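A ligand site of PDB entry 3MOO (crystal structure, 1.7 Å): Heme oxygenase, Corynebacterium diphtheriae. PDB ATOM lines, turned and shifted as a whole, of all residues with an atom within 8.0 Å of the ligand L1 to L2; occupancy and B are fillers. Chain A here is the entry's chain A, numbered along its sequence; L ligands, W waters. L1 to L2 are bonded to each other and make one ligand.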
ATOM      1  N   VAL A  10      -1.704 -19.966  28.463  1.00  0.00           N
ATOM      2  CA  VAL A  10      -2.309 -21.302  28.603  1.00  0.00           C
ATOM      3  C   VAL A  10      -3.066 -21.416  29.920  1.00  0.00           C
ATOM      4  O   VAL A  10      -4.176 -21.955  29.969  1.00  0.00           O
ATOM      5  CB  VAL A  10      -1.272 -22.446  28.477  1.00  0.00           C
ATOM      6  CG1 VAL A  10      -1.958 -23.811  28.753  1.00  0.00           C
ATOM      7  CG2 VAL A  10      -0.693 -22.474  27.094  1.00  0.00           C
ATOM      8  N   LEU A  12      -4.416 -19.116  31.715  1.00  0.00           N
ATOM      9  CA  LEU A  12      -5.635 -18.312  31.621  1.00  0.00           C
ATOM     10  C   LEU A  12      -6.735 -19.093  30.903  1.00  0.00           C
ATOM     11  O   LEU A  12      -7.883 -19.173  31.376  1.00  0.00           O
ATOM     12  CB  LEU A  12      -5.320 -17.040  30.858  1.00  0.00           C
ATOM     13  CG  LEU A  12      -5.900 -15.672  31.181  1.00  0.00           C
ATOM     14  CD1 LEU A  12      -6.378 -15.475  32.649  1.00  0.00           C
ATOM     15  CD2 LEU A  12      -4.874 -14.621  30.754  1.00  0.00           C
ATOM     16  N   LYS A  13      -6.388 -19.681  29.764  1.00  0.00           N
ATOM     17  CA  LYS A  13      -7.366 -20.447  28.973  1.00  0.00           C
ATOM     18  C   LYS A  13      -7.893 -21.634  29.780  1.00  0.00           C
ATOM     19  O   LYS A  13      -9.101 -21.909  29.789  1.00  0.00           O
ATOM     20  CB  LYS A  13      -6.730 -20.936  27.669  1.00  0.00           C
ATOM     21  CG  LYS A  13      -7.697 -21.552  26.656  1.00  0.00           C
ATOM     22  CD  LYS A  13      -6.900 -21.941  25.390  1.00  0.00           C
ATOM     23  CE  LYS A  13      -7.779 -22.405  24.226  1.00  0.00           C
ATOM     24  NZ  LYS A  13      -8.523 -23.636  24.573  1.00  0.00           N
ATOM     25  N   GLN A  14      -6.985 -22.306  30.496  1.00  0.00           N
ATOM     26  CA  GLN A  14      -7.389 -23.483  31.268  1.00  0.00           C
ATOM     27  C   GLN A  14      -8.187 -23.140  32.516  1.00  0.00           C
ATOM     28  O   GLN A  14      -9.207 -23.792  32.796  1.00  0.00           O
ATOM     29  CB  GLN A  14      -6.195 -24.357  31.602  1.00  0.00           C
ATOM     30  CG  GLN A  14      -5.521 -24.985  30.352  1.00  0.00           C
ATOM     31  CD  GLN A  14      -4.296 -25.795  30.682  1.00  0.00           C
ATOM     32  OE1 GLN A  14      -3.705 -25.674  31.753  1.00  0.00           O
ATOM     33  NE2 GLN A  14      -3.876 -26.618  29.730  1.00  0.00           N
ATOM     34  N   THR A  16     -10.110 -20.683  33.043  1.00  0.00           N
ATOM     35  CA  THR A  16     -11.428 -20.113  32.700  1.00  0.00           C
ATOM     36  C   THR A  16     -12.284 -21.028  31.788  1.00  0.00           C
ATOM     37  O   THR A  16     -13.398 -20.652  31.407  1.00  0.00           O
ATOM     38  CB  THR A  16     -11.274 -18.710  31.996  1.00  0.00           C
ATOM     39  OG1 THR A  16     -10.505 -18.876  30.792  1.00  0.00           O
ATOM     40  CG2 THR A  16     -10.551 -17.706  32.908  1.00  0.00           C
ATOM     41  N   ALA A  17     -11.774 -22.214  31.441  1.00  0.00           N
ATOM     42  CA  ALA A  17     -12.463 -23.131  30.496  1.00  0.00           C
ATOM     43  C   ALA A  17     -13.889 -23.445  30.926  1.00  0.00           C
ATOM     44  O   ALA A  17     -14.807 -23.392  30.118  1.00  0.00           O
ATOM     45  CB  ALA A  17     -11.661 -24.438  30.307  1.00  0.00           C
ATOM     46  N   GLN A  18     -14.074 -23.736  32.223  1.00  0.00           N
ATOM     47  CA  GLN A  18     -15.416 -24.039  32.757  1.00  0.00           C
ATOM     48  C   GLN A  18     -16.350 -22.818  32.676  1.00  0.00           C
ATOM     49  O   GLN A  18     -17.522 -22.951  32.285  1.00  0.00           O
ATOM     50  CB  GLN A  18     -15.321 -24.521  34.201  1.00  0.00           C
ATOM     51  CG  GLN A  18     -14.594 -25.853  34.387  1.00  0.00           C
ATOM     52  CD  GLN A  18     -15.439 -27.068  34.059  1.00  0.00           C
ATOM     53  OE1 GLN A  18     -16.072 -27.148  32.996  1.00  0.00           O
ATOM     54  NE2 GLN A  18     -15.425 -28.058  34.959  1.00  0.00           N
ATOM     55  N   ALA A  19     -15.806 -21.648  33.000  1.00  0.00           N
ATOM     56  CA  ALA A  19     -16.575 -20.402  32.958  1.00  0.00           C
ATOM     57  C   ALA A  19     -16.943 -20.028  31.533  1.00  0.00           C
ATOM     58  O   ALA A  19     -18.038 -19.542  31.283  1.00  0.00           O
ATOM     59  CB  ALA A  19     -15.851 -19.269  33.673  1.00  0.00           C
ATOM     60  N   HIS A  20     -16.022 -20.267  30.594  1.00  0.00           N
ATOM     61  CA  HIS A  20     -16.317 -20.086  29.165  1.00  0.00           C
ATOM     62  C   HIS A  20     -17.476 -20.950  28.695  1.00  0.00           C
ATOM     63  O   HIS A  20     -18.381 -20.478  28.024  1.00  0.00           O
ATOM     64  CB  HIS A  20     -15.098 -20.371  28.272  1.00  0.00           C
ATOM     65  CG  HIS A  20     -15.357 -20.098  26.825  1.00  0.00           C
ATOM     66  ND1 HIS A  20     -15.908 -21.019  25.966  1.00  0.00           N
ATOM     67  CD2 HIS A  20     -15.151 -18.975  26.095  1.00  0.00           C
ATOM     68  CE1 HIS A  20     -16.042 -20.487  24.757  1.00  0.00           C
ATOM     69  NE2 HIS A  20     -15.594 -19.241  24.806  1.00  0.00           N
ATOM     70  N   GLU A  21     -17.417 -22.242  29.014  1.00  0.00           N
ATOM     71  CA  GLU A  21     -18.502 -23.166  28.669  1.00  0.00           C
ATOM     72  C   GLU A  21     -19.856 -22.715  29.251  1.00  0.00           C
ATOM     73  O   GLU A  21     -20.881 -22.740  28.542  1.00  0.00           O
ATOM     74  CB  GLU A  21     -18.147 -24.590  29.117  1.00  0.00           C
ATOM     75  CG  GLU A  21     -19.191 -25.655  28.801  1.00  0.00           C
ATOM     76  CD  GLU A  21     -19.138 -26.205  27.357  1.00  0.00           C
ATOM     77  OE1 GLU A  21     -19.777 -27.252  27.138  1.00  0.00           O
ATOM     78  OE2 GLU A  21     -18.479 -25.615  26.453  1.00  0.00           O
ATOM     79  N   LYS A  22     -19.870 -22.311  30.514  1.00  0.00           N
ATOM     80  CA  LYS A  22     -21.089 -21.804  31.138  1.00  0.00           C
ATOM     81  C   LYS A  22     -21.619 -20.537  30.440  1.00  0.00           C
ATOM     82  O   LYS A  22     -22.828 -20.361  30.277  1.00  0.00           O
ATOM     83  CB  LYS A  22     -20.887 -21.572  32.639  1.00  0.00           C
ATOM     84  CG  LYS A  22     -22.101 -21.036  33.381  1.00  0.00           C
ATOM     85  CD  LYS A  22     -21.859 -21.061  34.882  1.00  0.00           C
ATOM     86  CE  LYS A  22     -23.167 -21.139  35.666  1.00  0.00           C
ATOM     87  NZ  LYS A  22     -22.949 -20.667  37.072  1.00  0.00           N
ATOM     88  N   ALA A  23     -20.706 -19.659  30.022  1.00  0.00           N
ATOM     89  CA  ALA A  23     -21.071 -18.411  29.307  1.00  0.00           C
ATOM     90  C   ALA A  23     -21.715 -18.728  27.969  1.00  0.00           C
ATOM     91  O   ALA A  23     -22.756 -18.167  27.606  1.00  0.00           O
ATOM     92  CB  ALA A  23     -19.815 -17.527  29.078  1.00  0.00           C
ATOM     93  N   GLU A  24     -21.074 -19.649  27.260  1.00  0.00           N
ATOM     94  CA  GLU A  24     -21.465 -20.065  25.941  1.00  0.00           C
ATOM     95  C   GLU A  24     -22.842 -20.743  25.949  1.00  0.00           C
ATOM     96  O   GLU A  24     -23.596 -20.586  25.002  1.00  0.00           O
ATOM     97  CB  GLU A  24     -20.376 -20.994  25.364  1.00  0.00           C
ATOM     98  CG  GLU A  24     -20.645 -21.535  23.972  1.00  0.00           C
ATOM     99  CD  GLU A  24     -19.629 -22.559  23.565  1.00  0.00           C
ATOM    100  OE1 GLU A  24     -19.997 -23.737  23.418  1.00  0.00           O
ATOM    101  OE2 GLU A  24     -18.448 -22.191  23.428  1.00  0.00           O
ATOM    102  N   HIS A  25     -23.166 -21.427  27.051  1.00  0.00           N
ATOM    103  CA  HIS A  25     -24.435 -22.180  27.164  1.00  0.00           C
ATOM    104  C   HIS A  25     -25.558 -21.523  28.004  1.00  0.00           C
ATOM    105  O   HIS A  25     -26.588 -22.140  28.277  1.00  0.00           O
ATOM    106  CB  HIS A  25     -24.170 -23.620  27.631  1.00  0.00           C
ATOM    107  CG  HIS A  25     -23.308 -24.409  26.706  1.00  0.00           C
ATOM    108  ND1 HIS A  25     -23.730 -24.819  25.457  1.00  0.00           N
ATOM    109  CD2 HIS A  25     -22.035 -24.842  26.833  1.00  0.00           C
ATOM    110  CE1 HIS A  25     -22.756 -25.483  24.867  1.00  0.00           C
ATOM    111  NE2 HIS A  25     -21.718 -25.506  25.671  1.00  0.00           N
ATOM    112  N   TYR A 130      -8.622  -9.354  28.377  1.00  0.00           N
ATOM    113  CA  TYR A 130      -8.533 -10.684  27.733  1.00  0.00           C
ATOM    114  C   TYR A 130      -9.929 -11.292  27.534  1.00  0.00           C
ATOM    115  O   TYR A 130     -10.264 -11.751  26.434  1.00  0.00           O
ATOM    116  CB  TYR A 130      -7.666 -11.596  28.603  1.00  0.00           C
ATOM    117  CG  TYR A 130      -7.877 -13.067  28.373  1.00  0.00           C
ATOM    118  CD1 TYR A 130      -7.271 -13.724  27.257  1.00  0.00           C
ATOM    119  CD2 TYR A 130      -8.632 -13.839  29.256  1.00  0.00           C
ATOM    120  CE1 TYR A 130      -7.413 -15.088  27.079  1.00  0.00           C
ATOM    121  CE2 TYR A 130      -8.797 -15.220  29.068  1.00  0.00           C
ATOM    122  CZ  TYR A 130      -8.201 -15.832  27.948  1.00  0.00           C
ATOM    123  OH  TYR A 130      -8.349 -17.190  27.781  1.00  0.00           O
ATOM    124  N   SER A 138     -12.954 -13.863  18.630  1.00  0.00           N
ATOM    125  CA  SER A 138     -13.078 -15.318  18.574  1.00  0.00           C
ATOM    126  C   SER A 138     -14.511 -15.659  18.239  1.00  0.00           C
ATOM    127  O   SER A 138     -14.915 -15.490  17.073  1.00  0.00           O
ATOM    128  CB  SER A 138     -12.602 -15.944  19.895  1.00  0.00           C
ATOM    129  OG  SER A 138     -11.193 -15.801  20.050  1.00  0.00           O
ATOM    130  N   GLY A 139     -15.282 -16.097  19.232  1.00  0.00           N
ATOM    131  CA  GLY A 139     -16.710 -16.394  19.059  1.00  0.00           C
ATOM    132  C   GLY A 139     -17.508 -15.199  18.564  1.00  0.00           C
ATOM    133  O   GLY A 139     -18.538 -15.374  17.912  1.00  0.00           O
ATOM    134  N   PHE A 201     -15.722 -13.550  33.450  1.00  0.00           N
ATOM    135  CA  PHE A 201     -16.652 -14.488  32.798  1.00  0.00           C
ATOM    136  C   PHE A 201     -17.962 -14.542  33.577  1.00  0.00           C
ATOM    137  O   PHE A 201     -19.047 -14.585  32.973  1.00  0.00           O
ATOM    138  CB  PHE A 201     -16.041 -15.887  32.720  1.00  0.00           C
ATOM    139  CG  PHE A 201     -15.280 -16.136  31.453  1.00  0.00           C
ATOM    140  CD1 PHE A 201     -15.952 -16.335  30.228  1.00  0.00           C
ATOM    141  CD2 PHE A 201     -13.888 -16.154  31.472  1.00  0.00           C
ATOM    142  CE1 PHE A 201     -15.216 -16.578  29.062  1.00  0.00           C
ATOM    143  CE2 PHE A 201     -13.149 -16.384  30.325  1.00  0.00           C
ATOM    144  CZ  PHE A 201     -13.806 -16.564  29.105  1.00  0.00           C
HETATM  145  C1  LIG L   1     -14.418 -26.780  24.748  1.00  0.00           C
HETATM  146  C2  LIG L   1     -14.252 -28.293  24.883  1.00  0.00           C
HETATM  147  C3  LIG L   1     -13.046 -28.731  24.080  1.00  0.00           C
HETATM  148  C4  LIG L   1     -13.164 -28.265  22.626  1.00  0.00           C
HETATM  149  C5  LIG L   1     -13.402 -26.757  22.565  1.00  0.00           C
HETATM  150  C6  LIG L   1     -13.597 -26.265  21.129  1.00  0.00           C
HETATM  151  O1  LIG L   1     -14.089 -28.625  26.265  1.00  0.00           O
HETATM  152  O2  LIG L   1     -12.941 -30.151  24.062  1.00  0.00           O
HETATM  153  O3  LIG L   1     -11.977 -28.670  21.963  1.00  0.00           O
HETATM  154  O4  LIG L   1     -14.576 -26.474  23.348  1.00  0.00           O
HETATM  155  O5  LIG L   1     -14.047 -24.897  21.056  1.00  0.00           O
HETATM  156  C1  LG2 L   2     -14.474 -25.074  27.144  1.00  0.00           C
HETATM  157  C2  LG2 L   2     -13.489 -24.900  25.990  1.00  0.00           C
HETATM  158  C3  LG2 L   2     -12.149 -24.375  26.493  1.00  0.00           C
HETATM  159  C4  LG2 L   2     -11.672 -23.550  25.323  1.00  0.00           C
HETATM  160  C5  LG2 L   2     -12.959 -22.890  24.855  1.00  0.00           C
HETATM  161  C6  LG2 L   2     -12.940 -22.389  23.410  1.00  0.00           C
HETATM  162  O1  LG2 L   2     -15.699 -24.443  26.775  1.00  0.00           O
HETATM  163  O2  LG2 L   2     -13.261 -26.141  25.301  1.00  0.00           O
HETATM  164  O3  LG2 L   2     -11.247 -25.456  26.796  1.00  0.00           O
HETATM  165  O4  LG2 L   2     -10.637 -22.617  25.674  1.00  0.00           O
HETATM  166  O5  LG2 L   2     -13.968 -23.891  25.066  1.00  0.00           O
HETATM  167  O6  LG2 L   2     -12.417 -23.406  22.540  1.00  0.00           O
HETATM  168  O1  LG3 L   3      -7.339 -18.155  25.631  1.00  0.00           O
HETATM  169  C1  LG3 L   3      -7.989 -18.416  24.593  1.00  0.00           C
HETATM  170  O2  LG3 L   3      -7.437 -18.680  23.517  1.00  0.00           O
HETATM  171  C2  LG3 L   3      -9.498 -18.400  24.644  1.00  0.00           C
HETATM  172  C3  LG3 L   3      -9.961 -17.119  23.961  1.00  0.00           C
HETATM  173  C4  LG3 L   3     -11.443 -16.891  24.212  1.00  0.00           C
HETATM  174  C5  LG3 L   3     -12.001 -16.021  25.131  1.00  0.00           C
HETATM  175  C6  LG3 L   3     -11.403 -15.085  26.172  1.00  0.00           C
HETATM  176  C7  LG3 L   3     -12.557 -17.524  23.499  1.00  0.00           C
HETATM  177  C8  LG3 L   3     -12.453 -18.482  22.473  1.00  0.00           C
HETATM  178  N1  LG3 L   3     -13.792 -17.179  24.156  1.00  0.00           N
HETATM  179  C9  LG3 L   3     -13.467 -16.109  25.033  1.00  0.00           C
HETATM  180  C10 LG3 L   3     -14.439 -15.448  25.714  1.00  0.00           C
HETATM  181  C11 LG3 L   3     -15.802 -15.606  25.537  1.00  0.00           C
HETATM  182  C12 LG3 L   3     -16.801 -14.888  26.322  1.00  0.00           C
HETATM  183  C13 LG3 L   3     -16.393 -13.902  27.358  1.00  0.00           C
HETATM  184  C14 LG3 L   3     -17.216 -12.912  27.675  1.00  0.00           C
HETATM  185  C15 LG3 L   3     -18.043 -15.246  25.966  1.00  0.00           C
HETATM  186  C16 LG3 L   3     -19.427 -14.818  26.414  1.00  0.00           C
HETATM  187 FE1  LG3 L   3     -15.509 -17.680  23.360  1.00  0.00          FE
HETATM  188  N2  LG3 L   3     -14.844 -18.891  21.954  1.00  0.00           N
HETATM  189  C17 LG3 L   3     -13.511 -19.115  21.788  1.00  0.00           C
HETATM  190  N3  LG3 L   3     -16.432 -16.367  24.601  1.00  0.00           N
HETATM  191  C18 LG3 L   3     -17.712 -16.208  24.963  1.00  0.00           C
HETATM  192  O3  LG3 L   3     -18.790 -16.716  24.399  1.00  0.00           O
HETATM  193  C19 LG3 L   3     -18.657 -17.519  23.413  1.00  0.00           C
HETATM  194  C20 LG3 L   3     -19.774 -18.172  22.755  1.00  0.00           C
HETATM  195  C21 LG3 L   3     -21.214 -17.911  22.972  1.00  0.00           C
HETATM  196  C22 LG3 L   3     -22.113 -18.835  22.698  1.00  0.00           C
HETATM  197  C23 LG3 L   3     -19.195 -18.964  21.854  1.00  0.00           C
HETATM  198  C24 LG3 L   3     -19.708 -19.948  20.793  1.00  0.00           C
HETATM  199  N4  LG3 L   3     -17.464 -17.984  23.212  1.00  0.00           N
HETATM  200  C25 LG3 L   3     -17.753 -18.805  22.077  1.00  0.00           C
HETATM  201  C26 LG3 L   3     -16.947 -19.605  21.236  1.00  0.00           C
HETATM  202  C27 LG3 L   3     -15.569 -19.672  21.161  1.00  0.00           C
HETATM  203  C28 LG3 L   3     -14.596 -20.430  20.341  1.00  0.00           C
HETATM  204  C29 LG3 L   3     -15.075 -21.401  19.272  1.00  0.00           C
HETATM  205  C30 LG3 L   3     -13.338 -20.076  20.709  1.00  0.00           C
HETATM  206  C31 LG3 L   3     -12.000 -20.619  20.171  1.00  0.00           C
HETATM  207  C32 LG3 L   3     -11.256 -19.577  19.341  1.00  0.00           C
HETATM  208  C33 LG3 L   3     -11.984 -19.278  18.050  1.00  0.00           C
HETATM  209  O4  LG3 L   3     -11.835 -18.167  17.520  1.00  0.00           O
HETATM  210  O5  LG3 L   3     -12.719 -20.157  17.538  1.00  0.00           O
HETATM  211  O   HOH W   1     -11.183 -21.181  28.077  1.00  0.00           O
HETATM  212  O   HOH W   2      -9.831 -24.194  21.923  1.00  0.00           O
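NE2 of His 20 is bound to FE1 of LG3 L3.
OE2 of Glu 21 is in hydrogen-bond range of O1 of LG2 L2 (3.0 Å).
NZ of Lys 13 is in hydrogen-bond range of O4 of LG2 L2 (2.6 Å).
The side-chain hydroxyl (OH) of Tyr 130 is in hydrogen-bond range of an oxygen (O1) of LG3 L3 (2.6 Å).
Water W2 lies within hydrogen-bond range of an oxygen (O6) of LG2 L2 (2.8 Å) and the side-chain amino group (NZ) of Lys 13 (3.0 Å).
Water W1 bridges the backbone carbonyl oxygen (O) of Lys 13 (2.8 Å) and an oxygen (O4) of LG2 L2 (2.9 Å).
Ala 17 touches the ligand L1 to L2.
ND1 of His 20 touches O1 of LG2 L2 (3.5 Å).
Hydrophobic or aromatic side chains within 4 Å of the ligand L1 to L2: Ala 17 and His 20.
Of the 18 residues printed, 4 come within 4 Å of the ligand L1 to L2.
The side-chain carboxylate (OE1) of Glu 21 sits at hydrogen-bond distance from a ring nitrogen (NE2) of His 25, at 3.0 Å.
O of Lys 13 lies within hydrogen-bond range of OG1 of Thr 16 (3.5 Å).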
